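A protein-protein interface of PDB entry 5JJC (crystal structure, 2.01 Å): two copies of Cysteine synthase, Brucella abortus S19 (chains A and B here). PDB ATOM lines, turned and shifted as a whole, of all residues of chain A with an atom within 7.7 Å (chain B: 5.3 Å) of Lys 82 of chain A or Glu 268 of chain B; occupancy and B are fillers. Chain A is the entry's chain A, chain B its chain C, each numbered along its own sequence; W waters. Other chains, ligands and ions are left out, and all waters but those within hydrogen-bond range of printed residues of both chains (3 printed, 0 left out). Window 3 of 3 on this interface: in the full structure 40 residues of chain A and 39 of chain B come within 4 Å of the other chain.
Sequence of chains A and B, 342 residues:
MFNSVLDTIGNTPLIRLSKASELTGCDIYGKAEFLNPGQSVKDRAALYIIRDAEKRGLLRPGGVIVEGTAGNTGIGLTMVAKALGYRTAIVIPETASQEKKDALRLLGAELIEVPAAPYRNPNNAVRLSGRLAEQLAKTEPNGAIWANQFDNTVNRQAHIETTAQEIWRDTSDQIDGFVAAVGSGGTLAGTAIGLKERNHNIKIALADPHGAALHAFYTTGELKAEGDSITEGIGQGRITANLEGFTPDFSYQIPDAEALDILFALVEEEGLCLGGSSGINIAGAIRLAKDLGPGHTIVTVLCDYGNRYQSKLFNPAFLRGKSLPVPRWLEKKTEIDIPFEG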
ATOM      1  N   VAL A   5      26.260  21.619 -25.050  1.00  0.00           N
ATOM      2  CA  VAL A   5      27.011  21.300 -26.291  1.00  0.00           C
ATOM      3  C   VAL A   5      26.131  21.598 -27.511  1.00  0.00           C
ATOM      4  O   VAL A   5      26.620  21.833 -28.608  1.00  0.00           O
ATOM      5  CB  VAL A   5      27.485  19.822 -26.303  1.00  0.00           C
ATOM      6  CG1 VAL A   5      26.284  18.883 -26.309  1.00  0.00           C
ATOM      7  CG2 VAL A   5      28.409  19.568 -27.460  1.00  0.00           C
ATOM      8  N   LEU A   6      24.820  21.657 -27.303  1.00  0.00           N
ATOM      9  CA  LEU A   6      23.917  21.905 -28.424  1.00  0.00           C
ATOM     10  C   LEU A   6      24.118  23.311 -28.998  1.00  0.00           C
ATOM     11  O   LEU A   6      23.844  23.548 -30.172  1.00  0.00           O
ATOM     12  CB  LEU A   6      22.458  21.720 -28.002  1.00  0.00           C
ATOM     13  CG  LEU A   6      22.055  20.363 -27.405  1.00  0.00           C
ATOM     14  CD1 LEU A   6      20.551  20.335 -27.156  1.00  0.00           C
ATOM     15  CD2 LEU A   6      22.449  19.218 -28.298  1.00  0.00           C
ATOM     16  N   ILE A  50      14.561  16.331 -32.886  1.00  0.00           N
ATOM     17  CA  ILE A  50      14.257  16.101 -31.486  1.00  0.00           C
ATOM     18  C   ILE A  50      13.501  17.284 -30.883  1.00  0.00           C
ATOM     19  O   ILE A  50      12.558  17.090 -30.119  1.00  0.00           O
ATOM     20  CB  ILE A  50      15.548  15.790 -30.692  1.00  0.00           C
ATOM     21  CG1 ILE A  50      16.052  14.405 -31.107  1.00  0.00           C
ATOM     22  CG2 ILE A  50      15.304  15.846 -29.188  1.00  0.00           C
ATOM     23  CD1 ILE A  50      17.413  14.034 -30.526  1.00  0.00           C
ATOM     24  N   ILE A  65      14.179   7.962 -28.776  1.00  0.00           N
ATOM     25  CA  ILE A  65      14.183   8.305 -30.190  1.00  0.00           C
ATOM     26  C   ILE A  65      14.677   7.097 -30.955  1.00  0.00           C
ATOM     27  O   ILE A  65      15.736   6.547 -30.651  1.00  0.00           O
ATOM     28  CB  ILE A  65      15.086   9.516 -30.486  1.00  0.00           C
ATOM     29  CG1 ILE A  65      14.578  10.743 -29.730  1.00  0.00           C
ATOM     30  CG2 ILE A  65      15.152   9.785 -31.987  1.00  0.00           C
ATOM     31  CD1 ILE A  65      15.614  11.358 -28.830  1.00  0.00           C
ATOM     32  N   GLY A  76      24.491  11.849 -34.287  1.00  0.00           N
ATOM     33  CA  GLY A  76      23.914  13.150 -34.003  1.00  0.00           C
ATOM     34  C   GLY A  76      22.734  13.058 -33.052  1.00  0.00           C
ATOM     35  O   GLY A  76      22.653  13.798 -32.069  1.00  0.00           O
ATOM     36  N   LEU A  77      21.808  12.149 -33.340  1.00  0.00           N
ATOM     37  CA  LEU A  77      20.623  11.974 -32.487  1.00  0.00           C
ATOM     38  C   LEU A  77      20.983  11.570 -31.054  1.00  0.00           C
ATOM     39  O   LEU A  77      20.377  12.047 -30.092  1.00  0.00           O
ATOM     40  CB  LEU A  77      19.688  10.915 -33.087  1.00  0.00           C
ATOM     41  CG  LEU A  77      18.868  11.271 -34.326  1.00  0.00           C
ATOM     42  CD1 LEU A  77      18.164  10.030 -34.868  1.00  0.00           C
ATOM     43  CD2 LEU A  77      17.857  12.369 -34.016  1.00  0.00           C
ATOM     44  N   THR A  78      21.962  10.679 -30.914  1.00  0.00           N
ATOM     45  CA  THR A  78      22.337  10.184 -29.586  1.00  0.00           C
ATOM     46  C   THR A  78      23.012  11.291 -28.755  1.00  0.00           C
ATOM     47  O   THR A  78      22.729  11.444 -27.562  1.00  0.00           O
ATOM     48  CB  THR A  78      23.251   8.945 -29.680  1.00  0.00           C
ATOM     49  OG1 THR A  78      22.559   7.904 -30.383  1.00  0.00           O
ATOM     50  CG2 THR A  78      23.599   8.422 -28.281  1.00  0.00           C
ATOM     51  N   MET A  79      23.881  12.079 -29.386  1.00  0.00           N
ATOM     52  CA  MET A  79      24.477  13.224 -28.688  1.00  0.00           C
ATOM     53  C   MET A  79      23.407  14.210 -28.214  1.00  0.00           C
ATOM     54  O   MET A  79      23.389  14.599 -27.046  1.00  0.00           O
ATOM     55  CB  MET A  79      25.480  13.953 -29.575  1.00  0.00           C
ATOM     56  CG  MET A  79      25.924  15.285 -28.983  1.00  0.00           C
ATOM     57  SD  MET A  79      26.880  16.221 -30.187  1.00  0.00           S
ATOM     58  CE  MET A  79      25.581  16.882 -31.228  1.00  0.00           C
ATOM     59  N   VAL A  80      22.508  14.604 -29.115  1.00  0.00           N
ATOM     60  CA  VAL A  80      21.412  15.505 -28.733  1.00  0.00           C
ATOM     61  C   VAL A  80      20.528  14.883 -27.647  1.00  0.00           C
ATOM     62  O   VAL A  80      20.192  15.541 -26.659  1.00  0.00           O
ATOM     63  CB  VAL A  80      20.553  15.893 -29.964  1.00  0.00           C
ATOM     64  CG1 VAL A  80      19.378  16.787 -29.561  1.00  0.00           C
ATOM     65  CG2 VAL A  80      21.424  16.599 -30.999  1.00  0.00           C
ATOM     66  N   ALA A  81      20.173  13.611 -27.814  1.00  0.00           N
ATOM     67  CA  ALA A  81      19.364  12.892 -26.819  1.00  0.00           C
ATOM     68  C   ALA A  81      19.972  12.933 -25.417  1.00  0.00           C
ATOM     69  O   ALA A  81      19.284  13.246 -24.438  1.00  0.00           O
ATOM     70  CB  ALA A  81      19.160  11.431 -27.253  1.00  0.00           C
ATOM     71  N   LYS A  82      21.260  12.608 -25.324  1.00  0.00           N
ATOM     72  CA  LYS A  82      21.950  12.583 -24.040  1.00  0.00           C
ATOM     73  C   LYS A  82      22.005  13.987 -23.439  1.00  0.00           C
ATOM     74  O   LYS A  82      21.815  14.161 -22.236  1.00  0.00           O
ATOM     75  CB  LYS A  82      23.362  12.003 -24.187  1.00  0.00           C
ATOM     76  CG  LYS A  82      23.407  10.512 -24.538  1.00  0.00           C
ATOM     77  CD  LYS A  82      22.587   9.661 -23.566  1.00  0.00           C
ATOM     78  CE  LYS A  82      22.455   8.222 -24.071  1.00  0.00           C
ATOM     79  NZ  LYS A  82      21.478   7.416 -23.252  1.00  0.00           N
ATOM     80  N   ALA A  83      22.246  14.994 -24.271  1.00  0.00           N
ATOM     81  CA  ALA A  83      22.231  16.368 -23.770  1.00  0.00           C
ATOM     82  C   ALA A  83      20.852  16.776 -23.218  1.00  0.00           C
ATOM     83  O   ALA A  83      20.762  17.647 -22.350  1.00  0.00           O
ATOM     84  CB  ALA A  83      22.676  17.337 -24.860  1.00  0.00           C
ATOM     85  N   LEU A  84      19.784  16.134 -23.687  1.00  0.00           N
ATOM     86  CA  LEU A  84      18.432  16.571 -23.320  1.00  0.00           C
ATOM     87  C   LEU A  84      17.656  15.587 -22.449  1.00  0.00           C
ATOM     88  O   LEU A  84      16.546  15.886 -22.025  1.00  0.00           O
ATOM     89  CB  LEU A  84      17.611  16.873 -24.581  1.00  0.00           C
ATOM     90  CG  LEU A  84      18.066  18.059 -25.426  1.00  0.00           C
ATOM     91  CD1 LEU A  84      17.233  18.150 -26.703  1.00  0.00           C
ATOM     92  CD2 LEU A  84      17.957  19.350 -24.629  1.00  0.00           C
ATOM     93  N   GLY A  85      18.226  14.420 -22.186  1.00  0.00           N
ATOM     94  CA  GLY A  85      17.613  13.476 -21.267  1.00  0.00           C
ATOM     95  C   GLY A  85      16.839  12.337 -21.912  1.00  0.00           C
ATOM     96  O   GLY A  85      15.968  11.733 -21.276  1.00  0.00           O
ATOM     97  N   TYR A  86      17.161  12.030 -23.167  1.00  0.00           N
ATOM     98  CA  TYR A  86      16.488  10.949 -23.878  1.00  0.00           C
ATOM     99  C   TYR A  86      17.441   9.788 -24.154  1.00  0.00           C
ATOM    100  O   TYR A  86      18.667   9.916 -23.993  1.00  0.00           O
ATOM    101  CB  TYR A  86      15.880  11.473 -25.190  1.00  0.00           C
ATOM    102  CG  TYR A  86      15.069  12.743 -25.005  1.00  0.00           C
ATOM    103  CD1 TYR A  86      13.925  12.751 -24.210  1.00  0.00           C
ATOM    104  CD2 TYR A  86      15.451  13.934 -25.616  1.00  0.00           C
ATOM    105  CE1 TYR A  86      13.187  13.913 -24.023  1.00  0.00           C
ATOM    106  CE2 TYR A  86      14.713  15.097 -25.442  1.00  0.00           C
ATOM    107  CZ  TYR A  86      13.580  15.079 -24.641  1.00  0.00           C
ATOM    108  OH  TYR A  86      12.845  16.238 -24.456  1.00  0.00           O
ATOM    109  N   ARG A  87      16.856   8.657 -24.538  1.00  0.00           N
ATOM    110  CA  ARG A  87      17.586   7.467 -24.965  1.00  0.00           C
ATOM    111  C   ARG A  87      17.420   7.345 -26.474  1.00  0.00           C
ATOM    112  O   ARG A  87      16.453   7.875 -27.031  1.00  0.00           O
ATOM    113  CB  ARG A  87      17.056   6.187 -24.290  1.00  0.00           C
ATOM    114  CG  ARG A  87      16.446   6.370 -22.901  1.00  0.00           C
ATOM    115  CD  ARG A  87      16.159   5.036 -22.183  1.00  0.00           C
ATOM    116  NE  ARG A  87      15.484   4.024 -23.004  1.00  0.00           N
ATOM    117  CZ  ARG A  87      14.165   3.809 -23.022  1.00  0.00           C
ATOM    118  NH1 ARG A  87      13.342   4.549 -22.283  1.00  0.00           N
ATOM    119  NH2 ARG A  87      13.663   2.863 -23.805  1.00  0.00           N
ATOM    120  N   THR A  88      18.337   6.647 -27.135  1.00  0.00           N
ATOM    121  CA  THR A  88      18.127   6.302 -28.539  1.00  0.00           C
ATOM    122  C   THR A  88      18.170   4.799 -28.777  1.00  0.00           C
ATOM    123  O   THR A  88      18.937   4.067 -28.145  1.00  0.00           O
ATOM    124  CB  THR A  88      19.170   6.947 -29.462  1.00  0.00           C
ATOM    125  OG1 THR A  88      20.482   6.564 -29.026  1.00  0.00           O
ATOM    126  CG2 THR A  88      19.035   8.473 -29.461  1.00  0.00           C
ATOM    127  N   LEU A 104      28.753   5.126 -31.929  1.00  0.00           N
ATOM    128  CA  LEU A 104      27.399   4.949 -31.404  1.00  0.00           C
ATOM    129  C   LEU A 104      27.384   4.267 -30.039  1.00  0.00           C
ATOM    130  O   LEU A 104      26.679   4.705 -29.121  1.00  0.00           O
ATOM    131  CB  LEU A 104      26.551   4.152 -32.398  1.00  0.00           C
ATOM    132  CG  LEU A 104      26.093   4.915 -33.651  1.00  0.00           C
ATOM    133  CD1 LEU A 104      25.658   3.933 -34.736  1.00  0.00           C
ATOM    134  CD2 LEU A 104      24.953   5.862 -33.291  1.00  0.00           C
ATOM    135  N   LEU A 106      29.903   4.077 -27.886  1.00  0.00           N
ATOM    136  CA  LEU A 106      30.535   5.005 -26.946  1.00  0.00           C
ATOM    137  C   LEU A 106      29.556   6.063 -26.442  1.00  0.00           C
ATOM    138  O   LEU A 106      29.520   6.369 -25.254  1.00  0.00           O
ATOM    139  CB  LEU A 106      31.751   5.701 -27.583  1.00  0.00           C
ATOM    140  CG  LEU A 106      33.111   5.258 -27.047  1.00  0.00           C
ATOM    141  CD1 LEU A 106      33.286   3.778 -27.328  1.00  0.00           C
ATOM    142  CD2 LEU A 106      34.213   6.068 -27.715  1.00  0.00           C
ATOM    143  N   LEU A 107      28.766   6.631 -27.346  1.00  0.00           N
ATOM    144  CA  LEU A 107      27.833   7.689 -26.960  1.00  0.00           C
ATOM    145  C   LEU A 107      26.628   7.180 -26.166  1.00  0.00           C
ATOM    146  O   LEU A 107      25.878   7.978 -25.586  1.00  0.00           O
ATOM    147  CB  LEU A 107      27.351   8.444 -28.202  1.00  0.00           C
ATOM    148  CG  LEU A 107      28.283   9.535 -28.727  1.00  0.00           C
ATOM    149  CD1 LEU A 107      27.724  10.130 -30.016  1.00  0.00           C
ATOM    150  CD2 LEU A 107      28.474  10.628 -27.689  1.00  0.00           C
ATOM    151  N   GLY A 108      26.432   5.865 -26.155  1.00  0.00           N
ATOM    152  CA  GLY A 108      25.367   5.260 -25.365  1.00  0.00           C
ATOM    153  C   GLY A 108      24.080   4.954 -26.115  1.00  0.00           C
ATOM    154  O   GLY A 108      23.016   4.802 -25.503  1.00  0.00           O
ATOM    155  N   ALA A 109      24.157   4.867 -27.440  1.00  0.00           N
ATOM    156  CA  ALA A 109      23.002   4.444 -28.219  1.00  0.00           C
ATOM    157  C   ALA A 109      22.726   2.976 -27.931  1.00  0.00           C
ATOM    158  O   ALA A 109      23.652   2.200 -27.689  1.00  0.00           O
ATOM    159  CB  ALA A 109      23.231   4.658 -29.710  1.00  0.00           C
ATOM    160  N   GLU A 110      21.454   2.598 -27.958  1.00  0.00           N
ATOM    161  CA  GLU A 110      21.105   1.188 -27.915  1.00  0.00           C
ATOM    162  C   GLU A 110      21.136   0.713 -29.355  1.00  0.00           C
ATOM    163  O   GLU A 110      20.297   1.091 -30.161  1.00  0.00           O
ATOM    164  CB  GLU A 110      19.736   0.961 -27.283  1.00  0.00           C
ATOM    165  CG  GLU A 110      19.307  -0.492 -27.305  1.00  0.00           C
ATOM    166  CD  GLU A 110      18.143  -0.766 -26.380  1.00  0.00           C
ATOM    167  OE1 GLU A 110      17.551   0.184 -25.859  1.00  0.00           O
ATOM    168  OE2 GLU A 110      17.806  -1.934 -26.155  1.00  0.00           O
ATOM    169  N   PHE B 264      32.365   9.608 -17.558  1.00  0.00           N
ATOM    170  CA  PHE B 264      31.302   8.706 -17.997  1.00  0.00           C
ATOM    171  C   PHE B 264      29.921   9.324 -17.777  1.00  0.00           C
ATOM    172  O   PHE B 264      29.053   9.232 -18.647  1.00  0.00           O
ATOM    173  CB  PHE B 264      31.432   7.353 -17.278  1.00  0.00           C
ATOM    174  CG  PHE B 264      32.715   6.614 -17.607  1.00  0.00           C
ATOM    175  CD1 PHE B 264      33.454   6.947 -18.738  1.00  0.00           C
ATOM    176  CD2 PHE B 264      33.180   5.599 -16.791  1.00  0.00           C
ATOM    177  CE1 PHE B 264      34.636   6.279 -19.043  1.00  0.00           C
ATOM    178  CE2 PHE B 264      34.359   4.924 -17.086  1.00  0.00           C
ATOM    179  CZ  PHE B 264      35.087   5.261 -18.215  1.00  0.00           C
ATOM    180  N   ALA B 265      29.734   9.972 -16.628  1.00  0.00           N
ATOM    181  CA  ALA B 265      28.507  10.716 -16.338  1.00  0.00           C
ATOM    182  C   ALA B 265      28.271  11.817 -17.374  1.00  0.00           C
ATOM    183  O   ALA B 265      27.139  12.081 -17.742  1.00  0.00           O
ATOM    184  CB  ALA B 265      28.566  11.321 -14.926  1.00  0.00           C
ATOM    185  N   LEU B 266      29.346  12.463 -17.827  1.00  0.00           N
ATOM    186  CA  LEU B 266      29.261  13.525 -18.824  1.00  0.00           C
ATOM    187  C   LEU B 266      28.663  13.017 -20.142  1.00  0.00           C
ATOM    188  O   LEU B 266      27.882  13.713 -20.785  1.00  0.00           O
ATOM    189  CB  LEU B 266      30.655  14.129 -19.063  1.00  0.00           C
ATOM    190  CG  LEU B 266      30.704  15.630 -19.364  1.00  0.00           C
ATOM    191  CD1 LEU B 266      30.159  16.461 -18.252  1.00  0.00           C
ATOM    192  CD2 LEU B 266      32.096  16.077 -19.635  1.00  0.00           C
ATOM    193  N   VAL B 267      29.048  11.814 -20.554  1.00  0.00           N
ATOM    194  CA  VAL B 267      28.450  11.206 -21.736  1.00  0.00           C
ATOM    195  C   VAL B 267      26.934  11.037 -21.548  1.00  0.00           C
ATOM    196  O   VAL B 267      26.144  11.472 -22.396  1.00  0.00           O
ATOM    197  CB  VAL B 267      29.069   9.823 -22.069  1.00  0.00           C
ATOM    198  CG1 VAL B 267      28.513   9.314 -23.405  1.00  0.00           C
ATOM    199  CG2 VAL B 267      30.589   9.874 -22.113  1.00  0.00           C
ATOM    200  N   GLU B 268      26.549  10.412 -20.432  1.00  0.00           N
ATOM    201  CA  GLU B 268      25.153  10.036 -20.138  1.00  0.00           C
ATOM    202  C   GLU B 268      24.229  11.216 -19.978  1.00  0.00           C
ATOM    203  O   GLU B 268      23.048  11.166 -20.367  1.00  0.00           O
ATOM    204  CB  GLU B 268      25.045   9.230 -18.830  1.00  0.00           C
ATOM    205  CG  GLU B 268      25.893   8.011 -18.744  1.00  0.00           C
ATOM    206  CD  GLU B 268      25.884   7.353 -17.358  1.00  0.00           C
ATOM    207  OE1 GLU B 268      26.006   6.113 -17.321  1.00  0.00           O
ATOM    208  OE2 GLU B 268      25.785   8.056 -16.321  1.00  0.00           O
ATOM    209  N   GLU B 269      24.776  12.263 -19.370  1.00  0.00           N
ATOM    210  CA  GLU B 269      23.998  13.381 -18.876  1.00  0.00           C
ATOM    211  C   GLU B 269      24.124  14.664 -19.695  1.00  0.00           C
ATOM    212  O   GLU B 269      23.210  15.495 -19.674  1.00  0.00           O
ATOM    213  CB  GLU B 269      24.406  13.665 -17.431  1.00  0.00           C
ATOM    214  CG  GLU B 269      24.121  12.524 -16.487  1.00  0.00           C
ATOM    215  CD  GLU B 269      24.662  12.787 -15.079  1.00  0.00           C
ATOM    216  OE1 GLU B 269      25.412  13.760 -14.875  1.00  0.00           O
ATOM    217  OE2 GLU B 269      24.327  12.027 -14.166  1.00  0.00           O
ATOM    218  N   GLU B 270      25.241  14.839 -20.409  1.00  0.00           N
ATOM    219  CA  GLU B 270      25.486  16.109 -21.091  1.00  0.00           C
ATOM    220  C   GLU B 270      25.898  15.947 -22.568  1.00  0.00           C
ATOM    221  O   GLU B 270      26.168  16.931 -23.249  1.00  0.00           O
ATOM    222  CB  GLU B 270      26.541  16.920 -20.297  1.00  0.00           C
ATOM    223  CG  GLU B 270      26.133  17.063 -18.809  1.00  0.00           C
ATOM    224  CD  GLU B 270      26.908  18.095 -17.994  1.00  0.00           C
ATOM    225  OE1 GLU B 270      27.304  19.147 -18.544  1.00  0.00           O
ATOM    226  OE2 GLU B 270      27.084  17.853 -16.780  1.00  0.00           O
ATOM    227  N   GLY B 271      25.908  14.714 -23.068  1.00  0.00           N
ATOM    228  CA  GLY B 271      26.192  14.466 -24.476  1.00  0.00           C
ATOM    229  C   GLY B 271      27.607  14.825 -24.908  1.00  0.00           C
ATOM    230  O   GLY B 271      27.835  15.174 -26.065  1.00  0.00           O
ATOM    231  N   ARG B 328      28.363   2.495 -17.360  1.00  0.00           N
ATOM    232  CA  ARG B 328      27.175   1.681 -17.096  1.00  0.00           C
ATOM    233  C   ARG B 328      26.515   1.186 -18.372  1.00  0.00           C
ATOM    234  O   ARG B 328      26.030   0.058 -18.422  1.00  0.00           O
ATOM    235  CB  ARG B 328      26.149   2.454 -16.257  1.00  0.00           C
ATOM    236  CG  ARG B 328      26.354   2.308 -14.761  1.00  0.00           C
ATOM    237  CD  ARG B 328      26.139   0.846 -14.304  1.00  0.00           C
ATOM    238  NE  ARG B 328      26.214   0.668 -12.846  1.00  0.00           N
ATOM    239  CZ  ARG B 328      27.324   0.796 -12.118  1.00  0.00           C
ATOM    240  NH1 ARG B 328      28.466   1.077 -12.693  1.00  0.00           N
ATOM    241  NH2 ARG B 328      27.314   0.630 -10.808  1.00  0.00           N
ATOM    242  N   TRP B 329      26.504   2.016 -19.407  1.00  0.00           N
ATOM    243  CA  TRP B 329      25.792   1.650 -20.620  1.00  0.00           C
ATOM    244  C   TRP B 329      26.527   0.603 -21.442  1.00  0.00           C
ATOM    245  O   TRP B 329      25.955   0.042 -22.364  1.00  0.00           O
ATOM    246  CB  TRP B 329      25.519   2.886 -21.481  1.00  0.00           C
ATOM    247  CG  TRP B 329      26.744   3.576 -22.032  1.00  0.00           C
ATOM    248  CD1 TRP B 329      27.312   3.390 -23.269  1.00  0.00           C
ATOM    249  CD2 TRP B 329      27.529   4.585 -21.379  1.00  0.00           C
ATOM    250  NE1 TRP B 329      28.401   4.215 -23.417  1.00  0.00           N
ATOM    251  CE2 TRP B 329      28.555   4.960 -22.275  1.00  0.00           C
ATOM    252  CE3 TRP B 329      27.464   5.207 -20.129  1.00  0.00           C
ATOM    253  CZ2 TRP B 329      29.510   5.925 -21.955  1.00  0.00           C
ATOM    254  CZ3 TRP B 329      28.423   6.162 -19.809  1.00  0.00           C
ATOM    255  CH2 TRP B 329      29.425   6.515 -20.724  1.00  0.00           C
HETATM  256  O   HOH W   1      20.724  12.468 -20.581  1.00  0.00           O
HETATM  257  O   HOH W   2      26.384  19.632 -23.005  1.00  0.00           O
HETATM  258  O   HOH W   3      22.495  17.938 -20.142  1.00  0.00           O
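The indole nitrogen of Trp 329 of chain B is in hydrogen-bond range of the backbone carbonyl oxygen of Leu 106 of chain A. O of Glu 269 of chain B lies close to O of Lys 82 of chain A, 3.2 Å away.
The backbone NH (N) of Gly 271 of chain B lies within hydrogen-bond range of the backbone carbonyl oxygen (O) of Leu 266 of chain B.
CG1 of Val 5 of chain A touches O of Glu 270 of chain B, 3.6 Å away. Gly 271 of chain B touches Met 79 of chain A (O to CG, 3.5 Å). CB of Lys 82 of chain A touches O of Val 267 of chain B, 3.4 Å away. N of Glu 270 of chain B touches O of Lys 82 of chain A, at 3.9 Å. Lys 82 of chain A touches Gly 271 of chain B (CB to CA, 3.8 Å). CB of Ala 83 of chain A touches O of Glu 270 of chain B, at 3.9 Å. N of Ala 83 of chain A touches N of Gly 271 of chain B, 3.9 Å away. CG1 of Val 267 of chain B touches O of Leu 106 of chain A, 3.6 Å away. Val 267 of chain B touches Leu 107 of chain A. CD1 of Trp 329 of chain B touches CA of Gly 108 of chain A, 3.4 Å away.
Printed residues of chain B within 4 Å of Met 79 of chain A: Gly 271. Lys 82 of chain A touches just these residues of chain B: Val 267 (3.4 Å), Glu 268 (3.6 Å), Glu 269 (3.2 Å), Glu 270 (3.9 Å) and Gly 271 (3.8 Å). Printed residues of chain B within 4 Å of Leu 107 of chain A: Val 267 (3.7 Å). Phe 264 of chain B touches none of the printed residues of chain A. Glu 268 of chain B touches just one residue of chain A: Lys 82 (3.6 Å). The nearest printed residue of chain A that does not touch Val 267 of chain B is Gly 108 of chain A (4.9 Å).
Of the 10 printed residues of chain B, 6 touch a printed residue of chain A. Printed residues of chain B that touch a printed residue of chain A: Val 267, Glu 268, Glu 269, Glu 270, Gly 271 and Trp 329. Hydrophobic or aromatic side chains of chain A that line the printed part of chain B: Val 5, Met 79 and Ala 83. Among the printed residues, no Asp or Glu carboxylate lies within 4 Å of a Lys or Arg side-chain nitrogen of the other chain.
No position is printed for both chains.
Water W3 lies within hydrogen-bond range of O of Glu 269 of chain B (2.6 Å) and O of Ala 83 of chain A (2.8 Å). Water W1 lies within hydrogen-bond range of the backbone carbonyl oxygen of Lys 82 of chain A and the backbone carbonyl oxygen of Glu 268 of chain B. Water W2 bridges O of Glu 270 of chain B (2.7 Å) and N of Val 5 of chain A (2.9 Å).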
